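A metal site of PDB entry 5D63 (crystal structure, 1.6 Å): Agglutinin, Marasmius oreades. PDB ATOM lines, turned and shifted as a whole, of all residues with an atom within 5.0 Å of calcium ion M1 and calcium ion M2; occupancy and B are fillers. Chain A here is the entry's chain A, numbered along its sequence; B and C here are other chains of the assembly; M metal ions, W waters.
Calcium ion M2 is bound by the side-chain carboxylate (OD1) of Asp 214 (2.3 Å). O of Gln 211 binds calcium ion M2 (2.4 Å). The side-chain carboxylate (OD2) of Asp 217 is bound to calcium ion M2. Water W2 is bound to calcium ion M2, at 2.4 Å. OD2 of Asp 216 is bound to calcium ion M2, 2.4 Å away. OD2 of Asp 183 of chain B is bound to calcium ion M2 (2.4 Å). OD1 of Asp 183 of chain B binds calcium ion M2.
Within 4 Å of calcium ion M1: Asp 214, Asp 216, Leu 182 of chain B, Asp 183 of chain B and Ala 3 of chain C. The nearest printed residue that does not touch calcium ion M1 is Asp 4 of chain C (4.03 Å).
Calcium ion M1 is bound by O of Leu 182 of chain B (2.3 Å). Calcium ion M1 is bound by OD1 of Asp 183 of chain B, 2.3 Å away. OD2 of Asp 214 binds calcium ion M1, 2.3 Å away. OD1 of Asp 216 binds calcium ion M1 (2.3 Å). The backbone carbonyl oxygen (O) of Ala 3 of chain C binds calcium ion M1. Water W1 is bound to calcium ion M1, 2.5 Å away.
Within 4 Å of calcium ion M2: Gln 211, Asp 214, Asp 216, Asp 217 and Asp 183 of chain B. Along chain A the residues within 4 Å of calcium ion M2 span positions 211 to 217.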
ATOM      1  N   GLN A 211      -1.184 -11.613   2.100  1.00  0.00           N
ATOM      2  CA  GLN A 211      -1.501 -11.003   3.395  1.00  0.00           C
ATOM      3  C   GLN A 211      -1.025  -9.551   3.634  1.00  0.00           C
ATOM      4  O   GLN A 211      -1.773  -8.747   4.178  1.00  0.00           O
ATOM      5  CB  GLN A 211      -1.064 -11.864   4.571  1.00  0.00           C
ATOM      6  CG  GLN A 211      -1.812 -13.251   4.629  1.00  0.00           C
ATOM      7  CD  GLN A 211      -1.664 -13.920   5.966  1.00  0.00           C
ATOM      8  OE1 GLN A 211      -1.914 -13.330   7.017  1.00  0.00           O
ATOM      9  NE2 GLN A 211      -1.307 -15.202   5.920  1.00  0.00           N
ATOM     10  N   ILE A 212       0.208  -9.241   3.253  1.00  0.00           N
ATOM     11  CA  ILE A 212       0.822  -7.919   3.588  1.00  0.00           C
ATOM     12  C   ILE A 212       0.300  -6.783   2.708  1.00  0.00           C
ATOM     13  O   ILE A 212       0.313  -5.625   3.118  1.00  0.00           O
ATOM     14  CB  ILE A 212       2.363  -8.069   3.523  1.00  0.00           C
ATOM     15  CG1 ILE A 212       3.122  -6.900   4.160  1.00  0.00           C
ATOM     16  CG2 ILE A 212       2.853  -8.354   2.111  1.00  0.00           C
ATOM     17  CD1 ILE A 212       2.946  -6.782   5.657  1.00  0.00           C
ATOM     18  N   TYR A 213      -0.121  -7.083   1.499  1.00  0.00           N
ATOM     19  CA  TYR A 213      -0.869  -6.077   0.705  1.00  0.00           C
ATOM     20  C   TYR A 213      -1.801  -6.763  -0.304  1.00  0.00           C
ATOM     21  O   TYR A 213      -1.534  -6.887  -1.500  1.00  0.00           O
ATOM     22  CB  TYR A 213       0.073  -5.030   0.087  1.00  0.00           C
ATOM     23  CG  TYR A 213      -0.560  -3.676   0.081  1.00  0.00           C
ATOM     24  CD1 TYR A 213      -0.565  -2.904   1.269  1.00  0.00           C
ATOM     25  CD2 TYR A 213      -1.131  -3.153  -1.092  1.00  0.00           C
ATOM     26  CE1 TYR A 213      -1.159  -1.688   1.254  1.00  0.00           C
ATOM     27  CE2 TYR A 213      -1.756  -1.954  -1.085  1.00  0.00           C
ATOM     28  CZ  TYR A 213      -1.723  -1.190   0.051  1.00  0.00           C
ATOM     29  OH  TYR A 213      -2.352   0.098   0.088  1.00  0.00           O
ATOM     30  N   ASP A 214      -2.806  -7.380   0.287  1.00  0.00           N
ATOM     31  CA  ASP A 214      -3.742  -8.210  -0.484  1.00  0.00           C
ATOM     32  C   ASP A 214      -5.092  -7.492  -0.573  1.00  0.00           C
ATOM     33  O   ASP A 214      -5.170  -6.249  -0.357  1.00  0.00           O
ATOM     34  CB  ASP A 214      -3.827  -9.669   0.064  1.00  0.00           C
ATOM     35  CG  ASP A 214      -4.444  -9.755   1.440  1.00  0.00           C
ATOM     36  OD1 ASP A 214      -4.339  -8.786   2.238  1.00  0.00           O
ATOM     37  OD2 ASP A 214      -4.945 -10.840   1.814  1.00  0.00           O
ATOM     38  N   ASP A 216      -7.884  -6.971   1.015  1.00  0.00           N
ATOM     39  CA  ASP A 216      -8.363  -6.116   2.074  1.00  0.00           C
ATOM     40  C   ASP A 216      -7.588  -4.809   2.166  1.00  0.00           C
ATOM     41  O   ASP A 216      -8.179  -3.722   2.429  1.00  0.00           O
ATOM     42  CB  ASP A 216      -8.395  -6.806   3.430  1.00  0.00           C
ATOM     43  CG  ASP A 216      -7.150  -7.644   3.702  1.00  0.00           C
ATOM     44  OD1 ASP A 216      -7.138  -8.837   3.285  1.00  0.00           O
ATOM     45  OD2 ASP A 216      -6.257  -7.064   4.355  1.00  0.00           O
ATOM     46  N   ASP A 217      -6.260  -4.903   1.956  1.00  0.00           N
ATOM     47  CA  ASP A 217      -5.463  -3.675   1.986  1.00  0.00           C
ATOM     48  C   ASP A 217      -5.835  -2.691   0.842  1.00  0.00           C
ATOM     49  O   ASP A 217      -5.943  -1.472   1.072  1.00  0.00           O
ATOM     50  CB  ASP A 217      -3.979  -4.016   1.909  1.00  0.00           C
ATOM     51  CG  ASP A 217      -3.558  -4.844   3.080  1.00  0.00           C
ATOM     52  OD1 ASP A 217      -3.396  -4.246   4.144  1.00  0.00           O
ATOM     53  OD2 ASP A 217      -3.481  -6.079   2.962  1.00  0.00           O
ATOM     54  N   LEU B 182      -9.456 -10.387   8.574  1.00  0.00           N
ATOM     55  CA  LEU B 182      -9.032 -10.124   7.246  1.00  0.00           C
ATOM     56  C   LEU B 182      -7.778 -10.905   6.762  1.00  0.00           C
ATOM     57  O   LEU B 182      -7.562 -11.063   5.544  1.00  0.00           O
ATOM     58  CB  LEU B 182      -8.736  -8.618   7.138  1.00  0.00           C
ATOM     59  CG  LEU B 182      -9.882  -7.650   7.477  1.00  0.00           C
ATOM     60  CD1 LEU B 182      -9.413  -6.178   7.473  1.00  0.00           C
ATOM     61  CD2 LEU B 182     -10.984  -7.731   6.550  1.00  0.00           C
ATOM     62  N   ASP B 183      -6.895 -11.348   7.684  1.00  0.00           N
ATOM     63  CA  ASP B 183      -5.672 -12.031   7.362  1.00  0.00           C
ATOM     64  C   ASP B 183      -5.446 -13.166   8.403  1.00  0.00           C
ATOM     65  O   ASP B 183      -6.385 -13.512   9.139  1.00  0.00           O
ATOM     66  CB  ASP B 183      -4.529 -10.967   7.404  1.00  0.00           C
ATOM     67  CG  ASP B 183      -4.606  -9.939   6.231  1.00  0.00           C
ATOM     68  OD1 ASP B 183      -4.651 -10.341   5.055  1.00  0.00           O
ATOM     69  OD2 ASP B 183      -4.547  -8.719   6.640  1.00  0.00           O
ATOM     70  N   ALA B 240       0.580 -10.127   7.923  1.00  0.00           N
ATOM     71  CA  ALA B 240       0.120  -8.777   7.957  1.00  0.00           C
ATOM     72  C   ALA B 240       0.580  -8.070   9.230  1.00  0.00           C
ATOM     73  O   ALA B 240       1.250  -8.671  10.067  1.00  0.00           O
ATOM     74  CB  ALA B 240      -1.382  -8.758   7.876  1.00  0.00           C
ATOM     75  N   VAL C   2     -12.077 -15.798   4.985  1.00  0.00           N
ATOM     76  CA  VAL C   2     -11.198 -14.596   5.145  1.00  0.00           C
ATOM     77  C   VAL C   2     -10.612 -14.156   3.798  1.00  0.00           C
ATOM     78  O   VAL C   2     -10.112 -14.955   2.999  1.00  0.00           O
ATOM     79  CB  VAL C   2     -10.168 -14.641   6.373  1.00  0.00           C
ATOM     80  CG1 VAL C   2     -10.300 -15.878   7.266  1.00  0.00           C
ATOM     81  CG2 VAL C   2      -8.732 -14.337   5.974  1.00  0.00           C
ATOM     82  N   ALA C   3     -10.733 -12.843   3.551  1.00  0.00           N
ATOM     83  CA  ALA C   3     -10.519 -12.314   2.210  1.00  0.00           C
ATOM     84  C   ALA C   3      -9.053 -12.305   1.800  1.00  0.00           C
ATOM     85  O   ALA C   3      -8.205 -11.811   2.502  1.00  0.00           O
ATOM     86  CB  ALA C   3     -11.134 -10.928   2.156  1.00  0.00           C
ATOM     87  N   ASP C   4      -8.725 -12.864   0.647  1.00  0.00           N
ATOM     88  CA  ASP C   4      -7.371 -12.600   0.094  1.00  0.00           C
ATOM     89  C   ASP C   4      -7.404 -11.838  -1.190  1.00  0.00           C
ATOM     90  O   ASP C   4      -6.373 -11.232  -1.569  1.00  0.00           O
ATOM     91  CB  ASP C   4      -6.594 -13.889  -0.069  1.00  0.00           C
ATOM     92  CG  ASP C   4      -7.248 -14.860  -1.072  1.00  0.00           C
ATOM     93  OD1 ASP C   4      -8.148 -14.454  -1.861  1.00  0.00           O
ATOM     94  OD2 ASP C   4      -6.831 -16.040  -1.046  1.00  0.00           O
HETATM   95 CA    CA M   1      -6.356 -10.990   3.643  1.00  0.00          CA
HETATM   96 CA    CA M   2      -3.986  -7.929   4.391  1.00  0.00          CA
HETATM   97  O   HOH W   1      -5.751 -13.359   3.893  1.00  0.00           O
HETATM   98  O   HOH W   2      -3.346  -6.208   5.940  1.00  0.00           O
